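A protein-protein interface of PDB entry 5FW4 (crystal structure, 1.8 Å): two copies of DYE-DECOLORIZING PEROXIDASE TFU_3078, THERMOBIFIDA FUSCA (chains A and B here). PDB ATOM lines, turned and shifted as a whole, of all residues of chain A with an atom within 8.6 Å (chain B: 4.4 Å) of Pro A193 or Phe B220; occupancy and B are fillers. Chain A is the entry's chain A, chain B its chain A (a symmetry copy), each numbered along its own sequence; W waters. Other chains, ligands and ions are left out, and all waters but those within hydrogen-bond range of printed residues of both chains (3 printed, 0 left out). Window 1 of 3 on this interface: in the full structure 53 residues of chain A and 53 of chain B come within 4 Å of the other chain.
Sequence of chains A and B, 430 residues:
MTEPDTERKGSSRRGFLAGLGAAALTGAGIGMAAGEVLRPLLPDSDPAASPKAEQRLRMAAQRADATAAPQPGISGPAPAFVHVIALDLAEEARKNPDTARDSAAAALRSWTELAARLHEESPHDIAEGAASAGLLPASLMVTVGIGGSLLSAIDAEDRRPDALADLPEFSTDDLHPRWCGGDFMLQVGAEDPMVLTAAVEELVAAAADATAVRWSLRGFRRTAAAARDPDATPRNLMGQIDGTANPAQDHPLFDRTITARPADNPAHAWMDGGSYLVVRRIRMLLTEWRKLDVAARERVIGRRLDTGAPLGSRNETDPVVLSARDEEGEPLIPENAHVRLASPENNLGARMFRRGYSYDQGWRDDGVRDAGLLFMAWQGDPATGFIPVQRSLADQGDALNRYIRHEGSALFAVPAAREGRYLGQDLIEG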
ATOM      1  N   ALA A  80       2.074 -12.911 -12.173  1.00  0.00           N
ATOM      2  CA  ALA A  80       2.718 -13.825 -11.270  1.00  0.00           C
ATOM      3  C   ALA A  80       4.209 -13.612 -10.916  1.00  0.00           C
ATOM      4  O   ALA A  80       4.655 -13.985  -9.845  1.00  0.00           O
ATOM      5  CB  ALA A  80       2.447 -15.228 -11.780  1.00  0.00           C
ATOM      6  N   PHE A  81       5.031 -13.079 -11.862  1.00  0.00           N
ATOM      7  CA  PHE A  81       6.463 -12.841 -11.608  1.00  0.00           C
ATOM      8  C   PHE A  81       6.896 -11.364 -11.701  1.00  0.00           C
ATOM      9  O   PHE A  81       6.325 -10.545 -12.420  1.00  0.00           O
ATOM     10  CB  PHE A  81       7.349 -13.691 -12.557  1.00  0.00           C
ATOM     11  CG  PHE A  81       6.991 -15.123 -12.558  1.00  0.00           C
ATOM     12  CD1 PHE A  81       5.940 -15.575 -13.311  1.00  0.00           C
ATOM     13  CD2 PHE A  81       7.651 -16.019 -11.700  1.00  0.00           C
ATOM     14  CE1 PHE A  81       5.604 -16.903 -13.281  1.00  0.00           C
ATOM     15  CE2 PHE A  81       7.302 -17.350 -11.651  1.00  0.00           C
ATOM     16  CZ  PHE A  81       6.259 -17.794 -12.433  1.00  0.00           C
ATOM     17  N   VAL A  82       7.909 -11.043 -10.924  1.00  0.00           N
ATOM     18  CA  VAL A  82       8.433  -9.710 -10.824  1.00  0.00           C
ATOM     19  C   VAL A  82       9.923  -9.817 -10.649  1.00  0.00           C
ATOM     20  O   VAL A  82      10.459 -10.806 -10.130  1.00  0.00           O
ATOM     21  CB  VAL A  82       7.793  -8.915  -9.660  1.00  0.00           C
ATOM     22  CG1 VAL A  82       8.448  -9.264  -8.335  1.00  0.00           C
ATOM     23  CG2 VAL A  82       7.879  -7.405  -9.918  1.00  0.00           C
ATOM     24  N   HIS A  83      10.616  -8.824 -11.196  1.00  0.00           N
ATOM     25  CA  HIS A  83      12.015  -8.622 -10.954  1.00  0.00           C
ATOM     26  C   HIS A  83      12.160  -7.144 -10.614  1.00  0.00           C
ATOM     27  O   HIS A  83      11.841  -6.258 -11.431  1.00  0.00           O
ATOM     28  CB  HIS A  83      12.867  -8.988 -12.210  1.00  0.00           C
ATOM     29  CG  HIS A  83      14.271  -9.308 -11.875  1.00  0.00           C
ATOM     30  ND1 HIS A  83      14.977 -10.294 -12.514  1.00  0.00           N
ATOM     31  CD2 HIS A  83      15.099  -8.810 -10.925  1.00  0.00           C
ATOM     32  CE1 HIS A  83      16.157 -10.414 -11.945  1.00  0.00           C
ATOM     33  NE2 HIS A  83      16.269  -9.490 -11.020  1.00  0.00           N
ATOM     34  N   ALA A 131      15.395 -15.371 -25.353  1.00  0.00           N
ATOM     35  CA  ALA A 131      15.124 -16.583 -24.598  1.00  0.00           C
ATOM     36  C   ALA A 131      13.641 -16.896 -24.649  1.00  0.00           C
ATOM     37  O   ALA A 131      13.227 -18.033 -24.471  1.00  0.00           O
ATOM     38  CB  ALA A 131      15.630 -16.433 -23.189  1.00  0.00           C
ATOM     39  N   SER A 132      12.860 -15.881 -24.955  1.00  0.00           N
ATOM     40  CA  SER A 132      11.399 -15.964 -24.933  1.00  0.00           C
ATOM     41  C   SER A 132      10.750 -16.299 -26.248  1.00  0.00           C
ATOM     42  O   SER A 132       9.510 -16.266 -26.375  1.00  0.00           O
ATOM     43  CB  SER A 132      10.843 -14.636 -24.387  1.00  0.00           C
ATOM     44  OG  SER A 132      11.249 -13.542 -25.167  1.00  0.00           O
ATOM     45  N   LEU A 135       6.971 -17.767 -27.167  1.00  0.00           N
ATOM     46  CA  LEU A 135       6.096 -17.610 -25.977  1.00  0.00           C
ATOM     47  C   LEU A 135       5.049 -16.498 -26.198  1.00  0.00           C
ATOM     48  O   LEU A 135       5.243 -15.589 -27.035  1.00  0.00           O
ATOM     49  CB  LEU A 135       6.953 -17.322 -24.759  1.00  0.00           C
ATOM     50  CG  LEU A 135       8.043 -18.336 -24.406  1.00  0.00           C
ATOM     51  CD1 LEU A 135       8.785 -17.917 -23.152  1.00  0.00           C
ATOM     52  CD2 LEU A 135       7.525 -19.751 -24.217  1.00  0.00           C
ATOM     53  N   ALA A 138       2.304 -12.677 -22.104  1.00  0.00           N
ATOM     54  CA  ALA A 138       2.403 -12.879 -20.632  1.00  0.00           C
ATOM     55  C   ALA A 138       2.368 -11.605 -19.836  1.00  0.00           C
ATOM     56  O   ALA A 138       3.142 -11.469 -18.874  1.00  0.00           O
ATOM     57  CB  ALA A 138       3.643 -13.682 -20.268  1.00  0.00           C
ATOM     58  N   GLY A 189       7.584  -7.040 -14.744  1.00  0.00           N
ATOM     59  CA  GLY A 189       6.623  -8.069 -14.387  1.00  0.00           C
ATOM     60  C   GLY A 189       6.154  -8.832 -15.591  1.00  0.00           C
ATOM     61  O   GLY A 189       6.004  -8.263 -16.685  1.00  0.00           O
ATOM     62  N   ALA A 190       5.986 -10.144 -15.411  1.00  0.00           N
ATOM     63  CA  ALA A 190       5.346 -10.951 -16.401  1.00  0.00           C
ATOM     64  C   ALA A 190       4.746 -12.194 -15.765  1.00  0.00           C
ATOM     65  O   ALA A 190       5.089 -12.559 -14.643  1.00  0.00           O
ATOM     66  CB  ALA A 190       6.323 -11.335 -17.538  1.00  0.00           C
ATOM     67  N   GLU A 191       3.824 -12.832 -16.485  1.00  0.00           N
ATOM     68  CA  GLU A 191       3.209 -14.056 -16.026  1.00  0.00           C
ATOM     69  C   GLU A 191       4.073 -15.288 -16.260  1.00  0.00           C
ATOM     70  O   GLU A 191       3.741 -16.358 -15.802  1.00  0.00           O
ATOM     71  CB  GLU A 191       1.837 -14.168 -16.712  1.00  0.00           C
ATOM     72  CG  GLU A 191       0.933 -15.270 -16.224  1.00  0.00           C
ATOM     73  CD  GLU A 191       0.438 -15.089 -14.779  1.00  0.00           C
ATOM     74  OE1 GLU A 191       0.373 -13.951 -14.265  1.00  0.00           O
ATOM     75  OE2 GLU A 191       0.048 -16.138 -14.266  1.00  0.00           O
ATOM     76  N   ASP A 192       5.156 -15.154 -17.046  1.00  0.00           N
ATOM     77  CA  ASP A 192       6.055 -16.262 -17.352  1.00  0.00           C
ATOM     78  C   ASP A 192       7.520 -15.841 -17.021  1.00  0.00           C
ATOM     79  O   ASP A 192       7.873 -14.697 -17.285  1.00  0.00           O
ATOM     80  CB  ASP A 192       5.958 -16.607 -18.853  1.00  0.00           C
ATOM     81  CG  ASP A 192       6.814 -17.742 -19.198  1.00  0.00           C
ATOM     82  OD1 ASP A 192       6.327 -18.861 -19.027  1.00  0.00           O
ATOM     83  OD2 ASP A 192       8.010 -17.510 -19.600  1.00  0.00           O
ATOM     84  N   PRO A 193       8.347 -16.713 -16.408  1.00  0.00           N
ATOM     85  CA  PRO A 193       9.622 -16.244 -15.902  1.00  0.00           C
ATOM     86  C   PRO A 193      10.610 -16.098 -17.084  1.00  0.00           C
ATOM     87  O   PRO A 193      11.610 -15.422 -16.988  1.00  0.00           O
ATOM     88  CB  PRO A 193      10.137 -17.383 -15.063  1.00  0.00           C
ATOM     89  CG  PRO A 193       9.450 -18.561 -15.570  1.00  0.00           C
ATOM     90  CD  PRO A 193       8.173 -18.138 -16.186  1.00  0.00           C
ATOM     91  N   MET A 194      10.334 -16.803 -18.129  1.00  0.00           N
ATOM     92  CA  MET A 194      11.231 -16.722 -19.297  1.00  0.00           C
ATOM     93  C   MET A 194      11.036 -15.443 -20.103  1.00  0.00           C
ATOM     94  O   MET A 194      12.032 -14.807 -20.601  1.00  0.00           O
ATOM     95  CB  MET A 194      11.020 -17.950 -20.185  1.00  0.00           C
ATOM     96  CG  MET A 194      12.155 -18.138 -21.157  1.00  0.00           C
ATOM     97  SD  MET A 194      13.767 -18.402 -20.388  1.00  0.00           S
ATOM     98  CE  MET A 194      13.928 -20.103 -19.939  1.00  0.00           C
ATOM     99  N   VAL A 195       9.771 -15.103 -20.329  1.00  0.00           N
ATOM    100  CA  VAL A 195       9.412 -13.792 -20.858  1.00  0.00           C
ATOM    101  C   VAL A 195      10.035 -12.697 -19.982  1.00  0.00           C
ATOM    102  O   VAL A 195      10.648 -11.771 -20.509  1.00  0.00           O
ATOM    103  CB  VAL A 195       7.896 -13.608 -20.995  1.00  0.00           C
ATOM    104  CG1 VAL A 195       7.531 -12.153 -21.352  1.00  0.00           C
ATOM    105  CG2 VAL A 195       7.256 -14.631 -21.930  1.00  0.00           C
ATOM    106  N   LEU A 196       9.858 -12.770 -18.636  1.00  0.00           N
ATOM    107  CA  LEU A 196      10.488 -11.856 -17.714  1.00  0.00           C
ATOM    108  C   LEU A 196      12.002 -11.658 -17.867  1.00  0.00           C
ATOM    109  O   LEU A 196      12.457 -10.541 -17.938  1.00  0.00           O
ATOM    110  CB  LEU A 196      10.137 -12.260 -16.234  1.00  0.00           C
ATOM    111  CG  LEU A 196      10.665 -11.366 -15.114  1.00  0.00           C
ATOM    112  CD1 LEU A 196      10.320  -9.908 -15.334  1.00  0.00           C
ATOM    113  CD2 LEU A 196      10.132 -11.784 -13.760  1.00  0.00           C
ATOM    114  N   THR A 197      12.776 -12.728 -17.886  1.00  0.00           N
ATOM    115  CA  THR A 197      14.224 -12.615 -17.822  1.00  0.00           C
ATOM    116  C   THR A 197      14.699 -12.086 -19.226  1.00  0.00           C
ATOM    117  O   THR A 197      15.679 -11.425 -19.287  1.00  0.00           O
ATOM    118  CB  THR A 197      14.899 -13.960 -17.495  1.00  0.00           C
ATOM    119  OG1 THR A 197      16.325 -13.818 -17.234  1.00  0.00           O
ATOM    120  CG2 THR A 197      14.714 -14.985 -18.592  1.00  0.00           C
ATOM    121  N   ALA A 198      13.923 -12.314 -20.262  1.00  0.00           N
ATOM    122  CA  ALA A 198      14.327 -11.848 -21.660  1.00  0.00           C
ATOM    123  C   ALA A 198      14.198 -10.341 -21.736  1.00  0.00           C
ATOM    124  O   ALA A 198      15.026  -9.625 -22.309  1.00  0.00           O
ATOM    125  CB  ALA A 198      13.413 -12.487 -22.665  1.00  0.00           C
ATOM    126  N   ALA A 199      13.130  -9.848 -21.131  1.00  0.00           N
ATOM    127  CA  ALA A 199      12.868  -8.430 -21.068  1.00  0.00           C
ATOM    128  C   ALA A 199      13.852  -7.742 -20.169  1.00  0.00           C
ATOM    129  O   ALA A 199      14.308  -6.676 -20.501  1.00  0.00           O
ATOM    130  CB  ALA A 199      11.442  -8.181 -20.574  1.00  0.00           C
ATOM    131  N   VAL A 200      14.068  -8.282 -18.957  1.00  0.00           N
ATOM    132  CA  VAL A 200      15.162  -7.786 -18.096  1.00  0.00           C
ATOM    133  C   VAL A 200      16.492  -7.627 -18.863  1.00  0.00           C
ATOM    134  O   VAL A 200      17.100  -6.606 -18.748  1.00  0.00           O
ATOM    135  CB  VAL A 200      15.413  -8.704 -16.943  1.00  0.00           C
ATOM    136  CG1 VAL A 200      16.722  -8.365 -16.231  1.00  0.00           C
ATOM    137  CG2 VAL A 200      14.219  -8.553 -15.987  1.00  0.00           C
ATOM    138  N   ARG A 218      14.192 -11.126  -7.544  1.00  0.00           N
ATOM    139  CA  ARG A 218      13.068 -11.715  -8.248  1.00  0.00           C
ATOM    140  C   ARG A 218      11.994 -12.193  -7.181  1.00  0.00           C
ATOM    141  O   ARG A 218      12.378 -12.739  -6.162  1.00  0.00           O
ATOM    142  CB  ARG A 218      13.581 -12.901  -9.003  1.00  0.00           C
ATOM    143  CG  ARG A 218      14.563 -12.484 -10.116  1.00  0.00           C
ATOM    144  CD  ARG A 218      15.029 -13.743 -10.775  1.00  0.00           C
ATOM    145  NE  ARG A 218      14.025 -14.355 -11.590  1.00  0.00           N
ATOM    146  CZ  ARG A 218      13.633 -15.616 -11.504  1.00  0.00           C
ATOM    147  NH1 ARG A 218      14.122 -16.424 -10.576  1.00  0.00           N
ATOM    148  NH2 ARG A 218      12.683 -16.053 -12.298  1.00  0.00           N
ATOM    149  N   GLY A 219      10.704 -12.065  -7.500  1.00  0.00           N
ATOM    150  CA  GLY A 219       9.592 -12.591  -6.662  1.00  0.00           C
ATOM    151  C   GLY A 219       8.521 -13.246  -7.507  1.00  0.00           C
ATOM    152  O   GLY A 219       8.542 -13.224  -8.754  1.00  0.00           O
ATOM    153  N   PHE A 220       7.574 -13.892  -6.853  1.00  0.00           N
ATOM    154  CA  PHE A 220       6.560 -14.648  -7.536  1.00  0.00           C
ATOM    155  C   PHE A 220       5.317 -14.665  -6.719  1.00  0.00           C
ATOM    156  O   PHE A 220       5.408 -14.439  -5.506  1.00  0.00           O
ATOM    157  CB  PHE A 220       6.992 -16.102  -7.835  1.00  0.00           C
ATOM    158  CG  PHE A 220       7.410 -16.906  -6.633  1.00  0.00           C
ATOM    159  CD1 PHE A 220       6.428 -17.598  -5.870  1.00  0.00           C
ATOM    160  CD2 PHE A 220       8.719 -16.898  -6.179  1.00  0.00           C
ATOM    161  CE1 PHE A 220       6.840 -18.352  -4.774  1.00  0.00           C
ATOM    162  CE2 PHE A 220       9.127 -17.632  -5.101  1.00  0.00           C
ATOM    163  CZ  PHE A 220       8.145 -18.330  -4.333  1.00  0.00           C
ATOM    164  N   THR A 223       0.758 -18.805 -10.093  1.00  0.00           N
ATOM    165  CA  THR A 223       0.404 -18.559 -11.501  1.00  0.00           C
ATOM    166  C   THR A 223      -1.105 -18.625 -11.675  1.00  0.00           C
ATOM    167  O   THR A 223      -1.814 -19.332 -10.919  1.00  0.00           O
ATOM    168  CB  THR A 223       1.121 -19.510 -12.514  1.00  0.00           C
ATOM    169  OG1 THR A 223       0.731 -20.884 -12.300  1.00  0.00           O
ATOM    170  CG2 THR A 223       2.590 -19.391 -12.410  1.00  0.00           C
ATOM    171  N   ALA B  80       7.755 -26.830 -15.423  1.00  0.00           N
ATOM    172  CA  ALA B  80       8.421 -25.563 -15.550  1.00  0.00           C
ATOM    173  C   ALA B  80       9.400 -25.108 -14.442  1.00  0.00           C
ATOM    174  O   ALA B  80      10.330 -24.364 -14.698  1.00  0.00           O
ATOM    175  CB  ALA B  80       7.354 -24.521 -15.832  1.00  0.00           C
ATOM    176  N   PHE B  81       9.148 -25.488 -13.158  1.00  0.00           N
ATOM    177  CA  PHE B  81      10.030 -25.102 -12.042  1.00  0.00           C
ATOM    178  C   PHE B  81      10.688 -26.284 -11.303  1.00  0.00           C
ATOM    179  O   PHE B  81      10.169 -27.397 -11.230  1.00  0.00           O
ATOM    180  CB  PHE B  81       9.277 -24.216 -11.015  1.00  0.00           C
ATOM    181  CG  PHE B  81       8.588 -23.067 -11.633  1.00  0.00           C
ATOM    182  CD1 PHE B  81       7.364 -23.228 -12.227  1.00  0.00           C
ATOM    183  CD2 PHE B  81       9.229 -21.819 -11.721  1.00  0.00           C
ATOM    184  CE1 PHE B  81       6.750 -22.157 -12.820  1.00  0.00           C
ATOM    185  CE2 PHE B  81       8.624 -20.746 -12.335  1.00  0.00           C
ATOM    186  CZ  PHE B  81       7.382 -20.919 -12.905  1.00  0.00           C
ATOM    187  N   GLY B 219      15.459 -23.267 -10.424  1.00  0.00           N
ATOM    188  CA  GLY B 219      15.507 -23.028 -11.893  1.00  0.00           C
ATOM    189  C   GLY B 219      14.121 -23.036 -12.503  1.00  0.00           C
ATOM    190  O   GLY B 219      13.101 -23.329 -11.847  1.00  0.00           O
ATOM    191  N   PHE B 220      14.037 -22.669 -13.767  1.00  0.00           N
ATOM    192  CA  PHE B 220      12.771 -22.528 -14.433  1.00  0.00           C
ATOM    193  C   PHE B 220      12.941 -22.801 -15.887  1.00  0.00           C
ATOM    194  O   PHE B 220      14.072 -22.697 -16.375  1.00  0.00           O
ATOM    195  CB  PHE B 220      12.146 -21.126 -14.249  1.00  0.00           C
ATOM    196  CG  PHE B 220      13.010 -19.976 -14.692  1.00  0.00           C
ATOM    197  CD1 PHE B 220      12.985 -19.556 -16.051  1.00  0.00           C
ATOM    198  CD2 PHE B 220      13.921 -19.385 -13.831  1.00  0.00           C
ATOM    199  CE1 PHE B 220      13.777 -18.478 -16.434  1.00  0.00           C
ATOM    200  CE2 PHE B 220      14.705 -18.330 -14.204  1.00  0.00           C
ATOM    201  CZ  PHE B 220      14.681 -17.903 -15.568  1.00  0.00           C
ATOM    202  N   ARG B 221      11.834 -23.158 -16.533  1.00  0.00           N
ATOM    203  CA  ARG B 221      11.732 -23.112 -17.988  1.00  0.00           C
ATOM    204  C   ARG B 221      10.483 -22.292 -18.296  1.00  0.00           C
ATOM    205  O   ARG B 221       9.771 -21.846 -17.349  1.00  0.00           O
ATOM    206  CB  ARG B 221      11.577 -24.499 -18.535  1.00  0.00           C
ATOM    207  CG  ARG B 221      12.673 -25.489 -18.230  1.00  0.00           C
ATOM    208  CD  ARG B 221      12.208 -26.903 -18.580  1.00  0.00           C
ATOM    209  NE  ARG B 221      13.331 -27.858 -18.592  1.00  0.00           N
ATOM    210  CZ  ARG B 221      13.363 -29.044 -19.204  1.00  0.00           C
ATOM    211  NH1 ARG B 221      12.318 -29.515 -19.839  1.00  0.00           N
ATOM    212  NH2 ARG B 221      14.455 -29.794 -19.114  1.00  0.00           N
ATOM    213  N   THR B 223       6.717 -21.571 -18.896  1.00  0.00           N
ATOM    214  CA  THR B 223       5.496 -22.243 -18.421  1.00  0.00           C
ATOM    215  C   THR B 223       4.715 -22.795 -19.603  1.00  0.00           C
ATOM    216  O   THR B 223       4.788 -22.260 -20.735  1.00  0.00           O
ATOM    217  CB  THR B 223       4.583 -21.345 -17.524  1.00  0.00           C
ATOM    218  OG1 THR B 223       4.081 -20.212 -18.266  1.00  0.00           O
ATOM    219  CG2 THR B 223       5.309 -20.871 -16.328  1.00  0.00           C
ATOM    220  N   TYR B 357      17.470 -26.782 -16.271  1.00  0.00           N
ATOM    221  CA  TYR B 357      16.649 -25.612 -16.021  1.00  0.00           C
ATOM    222  C   TYR B 357      17.514 -24.354 -16.093  1.00  0.00           C
ATOM    223  O   TYR B 357      18.679 -24.342 -15.642  1.00  0.00           O
ATOM    224  CB  TYR B 357      15.973 -25.736 -14.617  1.00  0.00           C
ATOM    225  CG  TYR B 357      14.843 -26.738 -14.625  1.00  0.00           C
ATOM    226  CD1 TYR B 357      15.098 -28.107 -14.600  1.00  0.00           C
ATOM    227  CD2 TYR B 357      13.523 -26.326 -14.779  1.00  0.00           C
ATOM    228  CE1 TYR B 357      14.061 -29.042 -14.671  1.00  0.00           C
ATOM    229  CE2 TYR B 357      12.498 -27.240 -14.861  1.00  0.00           C
ATOM    230  CZ  TYR B 357      12.765 -28.602 -14.804  1.00  0.00           C
ATOM    231  OH  TYR B 357      11.749 -29.501 -14.929  1.00  0.00           O
ATOM    232  N   SER B 358      16.929 -23.262 -16.549  1.00  0.00           N
ATOM    233  CA  SER B 358      17.537 -21.974 -16.387  1.00  0.00           C
ATOM    234  C   SER B 358      17.478 -21.479 -14.993  1.00  0.00           C
ATOM    235  O   SER B 358      16.589 -21.907 -14.248  1.00  0.00           O
ATOM    236  CB  SER B 358      16.842 -20.945 -17.274  1.00  0.00           C
ATOM    237  OG  SER B 358      17.080 -21.291 -18.631  1.00  0.00           O
ATOM    238  N   TYR B 359      18.422 -20.615 -14.654  1.00  0.00           N
ATOM    239  CA  TYR B 359      18.457 -19.893 -13.375  1.00  0.00           C
ATOM    240  C   TYR B 359      18.811 -18.473 -13.604  1.00  0.00           C
ATOM    241  O   TYR B 359      19.587 -18.126 -14.574  1.00  0.00           O
ATOM    242  CB  TYR B 359      19.402 -20.533 -12.349  1.00  0.00           C
ATOM    243  CG  TYR B 359      20.890 -20.401 -12.555  1.00  0.00           C
ATOM    244  CD1 TYR B 359      21.591 -19.338 -12.037  1.00  0.00           C
ATOM    245  CD2 TYR B 359      21.602 -21.379 -13.235  1.00  0.00           C
ATOM    246  CE1 TYR B 359      22.963 -19.246 -12.151  1.00  0.00           C
ATOM    247  CE2 TYR B 359      22.972 -21.301 -13.400  1.00  0.00           C
ATOM    248  CZ  TYR B 359      23.658 -20.217 -12.885  1.00  0.00           C
ATOM    249  OH  TYR B 359      25.028 -20.105 -13.047  1.00  0.00           O
ATOM    250  N   ASP B 360      18.184 -17.634 -12.804  1.00  0.00           N
ATOM    251  CA  ASP B 360      18.376 -16.198 -12.770  1.00  0.00           C
ATOM    252  C   ASP B 360      18.479 -15.772 -11.332  1.00  0.00           C
ATOM    253  O   ASP B 360      17.487 -15.812 -10.554  1.00  0.00           O
ATOM    254  CB  ASP B 360      17.252 -15.489 -13.506  1.00  0.00           C
ATOM    255  CG  ASP B 360      17.482 -13.961 -13.660  1.00  0.00           C
ATOM    256  OD1 ASP B 360      18.277 -13.353 -12.890  1.00  0.00           O
ATOM    257  OD2 ASP B 360      16.788 -13.348 -14.511  1.00  0.00           O
HETATM  258  O   HOH W   1      16.115 -15.866  -8.272  1.00  0.00           O
HETATM  259  O   HOH W   2       2.362 -18.693 -16.780  1.00  0.00           O
HETATM  260  O   HOH W   3      14.426 -12.413 -14.264  1.00  0.00           O
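The backbone carbonyl oxygen (O) of Ala A190 is in hydrogen-bond range of the backbone NH (N) of Phe A81.
The side-chain carboxylate (OD2) of Asp A192 lies within hydrogen-bond range of the backbone NH (N) of Met A194.
OD2 of Asp A192 sits at hydrogen-bond distance from N of Val A195, at 3.1 Å.
N of Arg B221 lies within hydrogen-bond range of O of Ala B80 (2.7 Å).
O of Ser B358 lies within hydrogen-bond range of N of Phe B220 (2.7 Å).
Phe B81 touches its own counterpart, Phe A81.
Positions printed for both chains: 80, 81, 219, 220 and 223.
Of the printed residues of chain B, His A83 touches Asp B360.
Of the printed residues of chain B, Asp A192 touches Thr B223.
Of the printed residues of chain B, Pro A193 touches Phe B81, Phe B220, Arg B221 and Thr B223.
Printed residues of chain B within 4 Å of Arg A218: Phe B220 and Asp B360.
Phe A220 touches none of the printed residues of chain B.
No residue of chain A comes within 4 Å of Gly B219.
Phe B220 touches just these residues of chain A: Pro A193, Met A194 and Arg A218.
Printed residues of chain A within 4 Å of Thr B223: Asp A192 and Pro A193.
Ser B358 touches just one residue of chain A: Met A194.
Hydrophobic or aromatic side chains of chain B within 4 Å of the printed part of chain A: Phe B81 and Phe B220.
Printed residues of chain A that touch a printed residue of chain B: Phe A81, His A83, Asp A192, Pro A193, Met A194, Thr A197 and Arg A218.
Hydrophobic or aromatic side chains of chain A that line the printed part of chain B: Phe A81, His A83, Pro A193 and Met A194.
Among the printed residues, 12 pairs touch across the chains.
OD1 of Asp A192 is in hydrogen-bond range of OG1 of Thr B223 (2.7 Å).
The side-chain carboxylate (OD2) of Asp B360 is in hydrogen-bond range of the side-chain hydroxyl (OG1) of Thr A197, 2.8 Å away.
The guanidinium group (NH1) of Arg A218 sits close to the backbone carbonyl oxygen (O) of Asp B360, at 3.4 Å.
Among the printed residues, merely in contact across the chains: Phe A81 with Phe B81, His A83 with Asp B360, Pro A193 with Phe B81, Pro A193 with Phe B220, Pro A193 with Arg B221, Pro A193 with Thr B223, Met A194 with Phe B220, Met A194 with Ser B358 and Arg A218 with Phe B220.
Water W3 lies within hydrogen-bond range of OD2 of Asp B360 (2.6 Å), ND1 of His A83 (2.8 Å) and NE of Arg A218 (3.3 Å).
Water W1 lies within hydrogen-bond range of the backbone carbonyl oxygen of Asp B360 and the guanidinium group of Arg A218.
Water W2 lies within hydrogen-bond range of the side-chain hydroxyl (OG1) of Thr B223 (2.7 Å) and the backbone carbonyl oxygen (O) of Glu A191 (2.9 Å).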
